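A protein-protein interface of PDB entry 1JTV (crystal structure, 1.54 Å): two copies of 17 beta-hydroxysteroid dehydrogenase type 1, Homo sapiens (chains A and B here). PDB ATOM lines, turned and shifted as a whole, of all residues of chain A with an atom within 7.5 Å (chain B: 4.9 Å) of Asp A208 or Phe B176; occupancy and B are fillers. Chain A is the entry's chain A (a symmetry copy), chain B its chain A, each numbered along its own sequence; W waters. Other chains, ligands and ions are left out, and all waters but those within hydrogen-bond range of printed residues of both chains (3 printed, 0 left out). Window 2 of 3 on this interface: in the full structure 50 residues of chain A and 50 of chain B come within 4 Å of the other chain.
The side-chain hydroxyl (OG1) of Thr A211 lies within hydrogen-bond range of the side-chain amino group (NZ) of Lys B130, 2.8 Å away. The side-chain amino group (NZ) of Lys B130 is in salt-bridge range of the side-chain carboxylate (OD1) of Asp A208 (3.9 Å). NZ of Lys B130 is in salt-bridge range of OE2 of Glu A100 (2.9 Å).
OD2 of Asp A208 is in hydrogen-bond range of N of His A210, 3.0 Å away. OD1 of Asp A208 sits at hydrogen-bond distance from OG1 of Thr A211 (2.6 Å). The side-chain hydroxyl (OG1) of Thr A207 lies within hydrogen-bond range of the side-chain carboxylate (OE2) of Glu A100.
Among the printed residues, merely in contact across the chains: Phe A151 with Leu B172 (3.5 Å), Asp A208 with Phe B176 (3.98 Å), Thr A211 with Phe B176 (3.3 Å), Arg A214 with Leu B172 (3.9 Å), Arg A214 with Pro B175 (3.95 Å), His A280 with Leu B174 (3.8 Å) and His A280 with Pro B175 (3.6 Å).
Printed residues of chain B within 4 Å of Glu A100: Lys B130. Printed residues of chain B within 4 Å of Asp A208: Lys B130 (3.9 Å) and Phe B176 (3.98 Å). Of the printed residues of chain B, Arg A214 touches Leu B172 and Pro B175. Printed residues of chain A within 4 Å of Leu B174: His A280 (3.8 Å). Of the printed residues of chain A, Pro B175 touches Arg A214 and His A280. Printed residues of chain A within 4 Å of Phe B176: Asp A208 and Thr A211. The nearest printed residue of chain A that does not touch Phe B176 is His A210 (4.2 Å). The nearest printed residue of chain B that does not touch Arg A214 is Phe B176 (4.9 Å).
Of the 16 printed residues of chain A, 6 touch a printed residue of chain B. Hydrophobic or aromatic side chains of chain A within 4 Å of the printed part of chain B: Phe A151 and His A280. Among the printed residues, 10 pairs touch across the chains.
No position is printed for both chains. Of the 10 pairs that touch across the chains among the printed residues, none has its exchanged pair printed and touching as well.
Water W1 lies within hydrogen-bond range of the backbone carbonyl oxygen (O) of Leu B172, a ring nitrogen (NE2) of His A280 and the guanidinium group (NE) of Arg A214. Water W2 bridges NZ of Lys B130 (2.8 Å) and OE1 of Glu A100 (2.9 Å). Water W3 bridges OD2 of Asp A208 (2.9 Å) and O of Lys B130 (3.3 Å).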
ATOM      1  N   PRO A  98       3.721 -11.756   8.349  1.00  0.00           N
ATOM      2  CA  PRO A  98       4.347 -12.973   8.854  1.00  0.00           C
ATOM      3  C   PRO A  98       3.402 -14.132   8.557  1.00  0.00           C
ATOM      4  O   PRO A  98       2.199 -14.020   8.806  1.00  0.00           O
ATOM      5  CB  PRO A  98       4.442 -12.722  10.358  1.00  0.00           C
ATOM      6  CG  PRO A  98       4.370 -11.238  10.529  1.00  0.00           C
ATOM      7  CD  PRO A  98       3.439 -10.772   9.429  1.00  0.00           C
ATOM      8  N   GLU A 100       2.580 -16.895  10.100  1.00  0.00           N
ATOM      9  CA  GLU A 100       1.766 -17.297  11.239  1.00  0.00           C
ATOM     10  C   GLU A 100       0.743 -16.251  11.679  1.00  0.00           C
ATOM     11  O   GLU A 100      -0.186 -16.533  12.463  1.00  0.00           O
ATOM     12  CB  GLU A 100       2.663 -17.700  12.421  1.00  0.00           C
ATOM     13  CG  GLU A 100       3.503 -16.543  12.926  1.00  0.00           C
ATOM     14  CD  GLU A 100       4.843 -16.406  12.259  1.00  0.00           C
ATOM     15  OE1 GLU A 100       5.049 -16.793  11.088  1.00  0.00           O
ATOM     16  OE2 GLU A 100       5.798 -15.908  12.902  1.00  0.00           O
ATOM     17  N   PHE A 151       7.781 -12.209   3.646  1.00  0.00           N
ATOM     18  CA  PHE A 151       6.498 -11.678   4.075  1.00  0.00           C
ATOM     19  C   PHE A 151       5.421 -11.647   3.002  1.00  0.00           C
ATOM     20  O   PHE A 151       4.315 -11.152   3.196  1.00  0.00           O
ATOM     21  CB  PHE A 151       6.719 -10.276   4.683  1.00  0.00           C
ATOM     22  CG  PHE A 151       7.558 -10.344   5.944  1.00  0.00           C
ATOM     23  CD1 PHE A 151       7.068 -10.984   7.060  1.00  0.00           C
ATOM     24  CD2 PHE A 151       8.832  -9.803   5.942  1.00  0.00           C
ATOM     25  CE1 PHE A 151       7.837 -11.026   8.227  1.00  0.00           C
ATOM     26  CE2 PHE A 151       9.597  -9.865   7.095  1.00  0.00           C
ATOM     27  CZ  PHE A 151       9.103 -10.489   8.224  1.00  0.00           C
ATOM     28  N   VAL A 203      -0.749  -7.667  14.119  1.00  0.00           N
ATOM     29  CA  VAL A 203       0.393  -8.448  13.651  1.00  0.00           C
ATOM     30  C   VAL A 203       1.294  -8.797  14.831  1.00  0.00           C
ATOM     31  O   VAL A 203       1.767  -9.917  14.983  1.00  0.00           O
ATOM     32  CB  VAL A 203       1.184  -7.719  12.555  1.00  0.00           C
ATOM     33  CG1 VAL A 203       2.426  -8.505  12.172  1.00  0.00           C
ATOM     34  CG2 VAL A 203       0.292  -7.497  11.332  1.00  0.00           C
ATOM     35  N   LEU A 204       1.540  -7.811  15.711  1.00  0.00           N
ATOM     36  CA  LEU A 204       2.368  -8.069  16.885  1.00  0.00           C
ATOM     37  C   LEU A 204       1.805  -9.169  17.772  1.00  0.00           C
ATOM     38  O   LEU A 204       2.557 -10.057  18.199  1.00  0.00           O
ATOM     39  CB  LEU A 204       2.565  -6.776  17.687  1.00  0.00           C
ATOM     40  CG  LEU A 204       3.451  -6.950  18.939  1.00  0.00           C
ATOM     41  CD1 LEU A 204       4.840  -7.436  18.576  1.00  0.00           C
ATOM     42  CD2 LEU A 204       3.475  -5.636  19.704  1.00  0.00           C
ATOM     43  N   ASP A 205       0.496  -9.235  17.967  1.00  0.00           N
ATOM     44  CA  ASP A 205      -0.125 -10.297  18.748  1.00  0.00           C
ATOM     45  C   ASP A 205      -0.017 -11.689  18.149  1.00  0.00           C
ATOM     46  O   ASP A 205      -0.161 -12.688  18.869  1.00  0.00           O
ATOM     47  CB  ASP A 205      -1.606  -9.962  18.966  1.00  0.00           C
ATOM     48  CG  ASP A 205      -1.837  -8.612  19.607  1.00  0.00           C
ATOM     49  OD1 ASP A 205      -0.939  -8.095  20.308  1.00  0.00           O
ATOM     50  OD2 ASP A 205      -2.935  -8.044  19.414  1.00  0.00           O
ATOM     51  N   ARG A 206       0.227 -11.821  16.841  1.00  0.00           N
ATOM     52  CA  ARG A 206       0.300 -13.131  16.216  1.00  0.00           C
ATOM     53  C   ARG A 206       1.691 -13.570  15.798  1.00  0.00           C
ATOM     54  O   ARG A 206       1.814 -14.561  15.059  1.00  0.00           O
ATOM     55  CB  ARG A 206      -0.631 -13.159  15.003  1.00  0.00           C
ATOM     56  CG  ARG A 206      -2.036 -12.650  15.282  1.00  0.00           C
ATOM     57  CD  ARG A 206      -2.999 -13.293  14.296  1.00  0.00           C
ATOM     58  NE  ARG A 206      -3.945 -12.322  13.760  1.00  0.00           N
ATOM     59  CZ  ARG A 206      -4.790 -12.627  12.775  1.00  0.00           C
ATOM     60  NH1 ARG A 206      -4.818 -13.843  12.245  1.00  0.00           N
ATOM     61  NH2 ARG A 206      -5.619 -11.692  12.332  1.00  0.00           N
ATOM     62  N   THR A 207       2.745 -12.844  16.177  1.00  0.00           N
ATOM     63  CA  THR A 207       4.081 -13.285  15.808  1.00  0.00           C
ATOM     64  C   THR A 207       5.075 -12.957  16.922  1.00  0.00           C
ATOM     65  O   THR A 207       4.676 -12.386  17.942  1.00  0.00           O
ATOM     66  CB  THR A 207       4.553 -12.737  14.454  1.00  0.00           C
ATOM     67  OG1 THR A 207       5.764 -13.399  14.076  1.00  0.00           O
ATOM     68  CG2 THR A 207       4.825 -11.243  14.546  1.00  0.00           C
ATOM     69  N   ASP A 208       6.333 -13.262  16.717  1.00  0.00           N
ATOM     70  CA  ASP A 208       7.352 -12.981  17.735  1.00  0.00           C
ATOM     71  C   ASP A 208       7.938 -11.604  17.471  1.00  0.00           C
ATOM     72  O   ASP A 208       7.850 -11.072  16.356  1.00  0.00           O
ATOM     73  CB  ASP A 208       8.441 -14.038  17.756  1.00  0.00           C
ATOM     74  CG  ASP A 208       9.219 -14.049  16.457  1.00  0.00           C
ATOM     75  OD1 ASP A 208       8.682 -14.708  15.532  1.00  0.00           O
ATOM     76  OD2 ASP A 208      10.265 -13.380  16.417  1.00  0.00           O
ATOM     77  N   ILE A 209       8.555 -10.995  18.482  1.00  0.00           N
ATOM     78  CA  ILE A 209       9.115  -9.658  18.322  1.00  0.00           C
ATOM     79  C   ILE A 209      10.175  -9.505  17.257  1.00  0.00           C
ATOM     80  O   ILE A 209      10.278  -8.419  16.644  1.00  0.00           O
ATOM     81  CB  ILE A 209       9.637  -9.159  19.703  1.00  0.00           C
ATOM     82  CG1 ILE A 209      10.008  -7.679  19.620  1.00  0.00           C
ATOM     83  CG2 ILE A 209      10.837  -9.956  20.181  1.00  0.00           C
ATOM     84  CD1 ILE A 209       8.813  -6.755  19.488  1.00  0.00           C
ATOM     85  N   HIS A 210      10.996 -10.522  16.974  1.00  0.00           N
ATOM     86  CA  HIS A 210      12.041 -10.467  15.977  1.00  0.00           C
ATOM     87  C   HIS A 210      11.405 -10.494  14.577  1.00  0.00           C
ATOM     88  O   HIS A 210      11.776  -9.672  13.739  1.00  0.00           O
ATOM     89  CB  HIS A 210      13.012 -11.651  16.115  1.00  0.00           C
ATOM     90  CG  HIS A 210      13.543 -11.704  17.525  1.00  0.00           C
ATOM     91  ND1 HIS A 210      14.349 -10.699  18.012  1.00  0.00           N
ATOM     92  CD2 HIS A 210      13.369 -12.592  18.522  1.00  0.00           C
ATOM     93  CE1 HIS A 210      14.655 -10.984  19.276  1.00  0.00           C
ATOM     94  NE2 HIS A 210      14.080 -12.126  19.600  1.00  0.00           N
ATOM     95  N   THR A 211      10.441 -11.405  14.413  1.00  0.00           N
ATOM     96  CA  THR A 211       9.760 -11.417  13.100  1.00  0.00           C
ATOM     97  C   THR A 211       9.059 -10.083  12.858  1.00  0.00           C
ATOM     98  O   THR A 211       9.095  -9.532  11.748  1.00  0.00           O
ATOM     99  CB  THR A 211       8.730 -12.553  13.010  1.00  0.00           C
ATOM    100  OG1 THR A 211       9.463 -13.790  13.173  1.00  0.00           O
ATOM    101  CG2 THR A 211       8.022 -12.526  11.663  1.00  0.00           C
ATOM    102  N   PHE A 212       8.436  -9.540  13.893  1.00  0.00           N
ATOM    103  CA  PHE A 212       7.768  -8.243  13.801  1.00  0.00           C
ATOM    104  C   PHE A 212       8.733  -7.150  13.376  1.00  0.00           C
ATOM    105  O   PHE A 212       8.435  -6.319  12.499  1.00  0.00           O
ATOM    106  CB  PHE A 212       7.059  -7.918  15.114  1.00  0.00           C
ATOM    107  CG  PHE A 212       6.259  -6.650  15.058  1.00  0.00           C
ATOM    108  CD1 PHE A 212       4.938  -6.669  14.649  1.00  0.00           C
ATOM    109  CD2 PHE A 212       6.835  -5.430  15.389  1.00  0.00           C
ATOM    110  CE1 PHE A 212       4.194  -5.500  14.588  1.00  0.00           C
ATOM    111  CE2 PHE A 212       6.100  -4.265  15.328  1.00  0.00           C
ATOM    112  CZ  PHE A 212       4.774  -4.300  14.930  1.00  0.00           C
ATOM    113  N   HIS A 213       9.915  -7.082  13.982  1.00  0.00           N
ATOM    114  CA  HIS A 213      10.931  -6.107  13.615  1.00  0.00           C
ATOM    115  C   HIS A 213      11.388  -6.270  12.174  1.00  0.00           C
ATOM    116  O   HIS A 213      11.546  -5.313  11.416  1.00  0.00           O
ATOM    117  CB  HIS A 213      12.106  -6.270  14.590  1.00  0.00           C
ATOM    118  CG  HIS A 213      13.330  -5.496  14.217  1.00  0.00           C
ATOM    119  ND1 HIS A 213      13.590  -4.221  14.665  1.00  0.00           N
ATOM    120  CD2 HIS A 213      14.379  -5.838  13.431  1.00  0.00           C
ATOM    121  CE1 HIS A 213      14.766  -3.841  14.177  1.00  0.00           C
ATOM    122  NE2 HIS A 213      15.251  -4.791  13.414  1.00  0.00           N
ATOM    123  N   ARG A 214      11.533  -7.534  11.743  1.00  0.00           N
ATOM    124  CA  ARG A 214      11.921  -7.807  10.362  1.00  0.00           C
ATOM    125  C   ARG A 214      10.810  -7.374   9.412  1.00  0.00           C
ATOM    126  O   ARG A 214      11.097  -6.928   8.289  1.00  0.00           O
ATOM    127  CB  ARG A 214      12.223  -9.302  10.212  1.00  0.00           C
ATOM    128  CG  ARG A 214      13.555  -9.723  10.798  1.00  0.00           C
ATOM    129  CD  ARG A 214      14.735  -8.984  10.208  1.00  0.00           C
ATOM    130  NE  ARG A 214      15.991  -9.644  10.543  1.00  0.00           N
ATOM    131  CZ  ARG A 214      17.215  -9.243  10.259  1.00  0.00           C
ATOM    132  NH1 ARG A 214      17.451  -8.105   9.621  1.00  0.00           N
ATOM    133  NH2 ARG A 214      18.232 -10.014  10.637  1.00  0.00           N
ATOM    134  N   HIS A 280      18.086 -11.795   1.136  1.00  0.00           N
ATOM    135  CA  HIS A 280      18.053 -11.405   2.552  1.00  0.00           C
ATOM    136  C   HIS A 280      18.836 -10.092   2.693  1.00  0.00           C
ATOM    137  O   HIS A 280      18.375  -9.155   3.346  1.00  0.00           O
ATOM    138  CB  HIS A 280      18.637 -12.488   3.468  1.00  0.00           C
ATOM    139  CG  HIS A 280      18.402 -12.157   4.910  1.00  0.00           C
ATOM    140  ND1 HIS A 280      19.256 -11.333   5.637  1.00  0.00           N
ATOM    141  CD2 HIS A 280      17.412 -12.505   5.759  1.00  0.00           C
ATOM    142  CE1 HIS A 280      18.777 -11.196   6.856  1.00  0.00           C
ATOM    143  NE2 HIS A 280      17.652 -11.890   6.962  1.00  0.00           N
ATOM    144  N   LYS B 130      11.040 -21.056  15.638  1.00  0.00           N
ATOM    145  CA  LYS B 130      11.641 -19.714  15.630  1.00  0.00           C
ATOM    146  C   LYS B 130      11.998 -19.269  17.045  1.00  0.00           C
ATOM    147  O   LYS B 130      13.062 -18.659  17.228  1.00  0.00           O
ATOM    148  CB  LYS B 130      10.681 -18.722  14.962  1.00  0.00           C
ATOM    149  CG  LYS B 130      10.462 -18.995  13.478  1.00  0.00           C
ATOM    150  CD  LYS B 130       9.243 -18.240  12.947  1.00  0.00           C
ATOM    151  CE  LYS B 130       9.645 -16.960  12.253  1.00  0.00           C
ATOM    152  NZ  LYS B 130       8.459 -16.125  11.890  1.00  0.00           N
ATOM    153  N   GLY B 133      15.040 -21.287  18.125  1.00  0.00           N
ATOM    154  CA  GLY B 133      16.146 -20.973  17.253  1.00  0.00           C
ATOM    155  C   GLY B 133      16.730 -22.243  16.636  1.00  0.00           C
ATOM    156  O   GLY B 133      17.912 -22.326  16.346  1.00  0.00           O
ATOM    157  N   SER B 134      15.864 -23.243  16.440  1.00  0.00           N
ATOM    158  CA  SER B 134      16.317 -24.498  15.849  1.00  0.00           C
ATOM    159  C   SER B 134      15.098 -25.254  15.312  1.00  0.00           C
ATOM    160  O   SER B 134      13.955 -25.071  15.735  1.00  0.00           O
ATOM    161  CB  SER B 134      17.059 -25.389  16.837  1.00  0.00           C
ATOM    162  OG  SER B 134      16.200 -25.788  17.886  1.00  0.00           O
ATOM    163  N   LEU B 172      13.316 -15.110   4.955  1.00  0.00           N
ATOM    164  CA  LEU B 172      13.142 -14.612   6.323  1.00  0.00           C
ATOM    165  C   LEU B 172      13.847 -15.463   7.362  1.00  0.00           C
ATOM    166  O   LEU B 172      14.494 -14.958   8.291  1.00  0.00           O
ATOM    167  CB  LEU B 172      11.649 -14.523   6.649  1.00  0.00           C
ATOM    168  CG  LEU B 172      11.311 -14.217   8.110  1.00  0.00           C
ATOM    169  CD1 LEU B 172      11.761 -12.790   8.474  1.00  0.00           C
ATOM    170  CD2 LEU B 172       9.827 -14.420   8.336  1.00  0.00           C
ATOM    171  N   LEU B 173      13.723 -16.790   7.248  1.00  0.00           N
ATOM    172  CA  LEU B 173      14.259 -17.703   8.246  1.00  0.00           C
ATOM    173  C   LEU B 173      15.767 -17.810   8.323  1.00  0.00           C
ATOM    174  O   LEU B 173      16.261 -18.326   9.330  1.00  0.00           O
ATOM    175  CB  LEU B 173      13.646 -19.100   8.011  1.00  0.00           C
ATOM    176  CG  LEU B 173      12.135 -19.237   8.192  1.00  0.00           C
ATOM    177  CD1 LEU B 173      11.680 -20.657   7.846  1.00  0.00           C
ATOM    178  CD2 LEU B 173      11.697 -18.886   9.608  1.00  0.00           C
ATOM    179  N   LEU B 174      16.522 -17.300   7.366  1.00  0.00           N
ATOM    180  CA  LEU B 174      17.972 -17.383   7.302  1.00  0.00           C
ATOM    181  C   LEU B 174      18.686 -17.214   8.640  1.00  0.00           C
ATOM    182  O   LEU B 174      19.385 -18.149   9.054  1.00  0.00           O
ATOM    183  CB  LEU B 174      18.527 -16.468   6.218  1.00  0.00           C
ATOM    184  CG  LEU B 174      20.021 -16.538   5.891  1.00  0.00           C
ATOM    185  CD1 LEU B 174      20.461 -17.950   5.537  1.00  0.00           C
ATOM    186  CD2 LEU B 174      20.360 -15.585   4.751  1.00  0.00           C
ATOM    187  N   PRO B 175      18.524 -16.098   9.329  1.00  0.00           N
ATOM    188  CA  PRO B 175      19.164 -15.875  10.617  1.00  0.00           C
ATOM    189  C   PRO B 175      18.468 -16.451  11.833  1.00  0.00           C
ATOM    190  O   PRO B 175      18.994 -16.332  12.960  1.00  0.00           O
ATOM    191  CB  PRO B 175      19.191 -14.345  10.716  1.00  0.00           C
ATOM    192  CG  PRO B 175      17.987 -13.900   9.966  1.00  0.00           C
ATOM    193  CD  PRO B 175      17.753 -14.915   8.873  1.00  0.00           C
ATOM    194  N   PHE B 176      17.324 -17.118  11.733  1.00  0.00           N
ATOM    195  CA  PHE B 176      16.599 -17.652  12.874  1.00  0.00           C
ATOM    196  C   PHE B 176      17.143 -19.000  13.349  1.00  0.00           C
ATOM    197  O   PHE B 176      16.725 -19.457  14.426  1.00  0.00           O
ATOM    198  CB  PHE B 176      15.105 -17.812  12.571  1.00  0.00           C
ATOM    199  CG  PHE B 176      14.257 -16.575  12.635  1.00  0.00           C
ATOM    200  CD1 PHE B 176      14.207 -15.693  11.570  1.00  0.00           C
ATOM    201  CD2 PHE B 176      13.502 -16.306  13.771  1.00  0.00           C
ATOM    202  CE1 PHE B 176      13.428 -14.547  11.631  1.00  0.00           C
ATOM    203  CE2 PHE B 176      12.712 -15.167  13.832  1.00  0.00           C
ATOM    204  CZ  PHE B 176      12.675 -14.295  12.761  1.00  0.00           C
ATOM    205  N   GLY B 177      17.987 -19.652  12.549  1.00  0.00           N
ATOM    206  CA  GLY B 177      18.475 -20.981  12.967  1.00  0.00           C
ATOM    207  C   GLY B 177      17.515 -22.105  12.554  1.00  0.00           C
ATOM    208  O   GLY B 177      17.705 -23.278  12.874  1.00  0.00           O
ATOM    209  N   VAL B 178      16.450 -21.728  11.855  1.00  0.00           N
ATOM    210  CA  VAL B 178      15.420 -22.670  11.404  1.00  0.00           C
ATOM    211  C   VAL B 178      15.717 -22.928   9.933  1.00  0.00           C
ATOM    212  O   VAL B 178      15.846 -21.978   9.169  1.00  0.00           O
ATOM    213  CB  VAL B 178      14.015 -22.112  11.606  1.00  0.00           C
ATOM    214  CG1 VAL B 178      12.946 -23.094  11.119  1.00  0.00           C
ATOM    215  CG2 VAL B 178      13.766 -21.871  13.098  1.00  0.00           C
HETATM  216  O   HOH W   1      15.403 -12.479   8.893  1.00  0.00           O
HETATM  217  O   HOH W   2       7.392 -16.692   9.355  1.00  0.00           O
HETATM  218  O   HOH W   3      11.818 -15.598  17.579  1.00  0.00           O
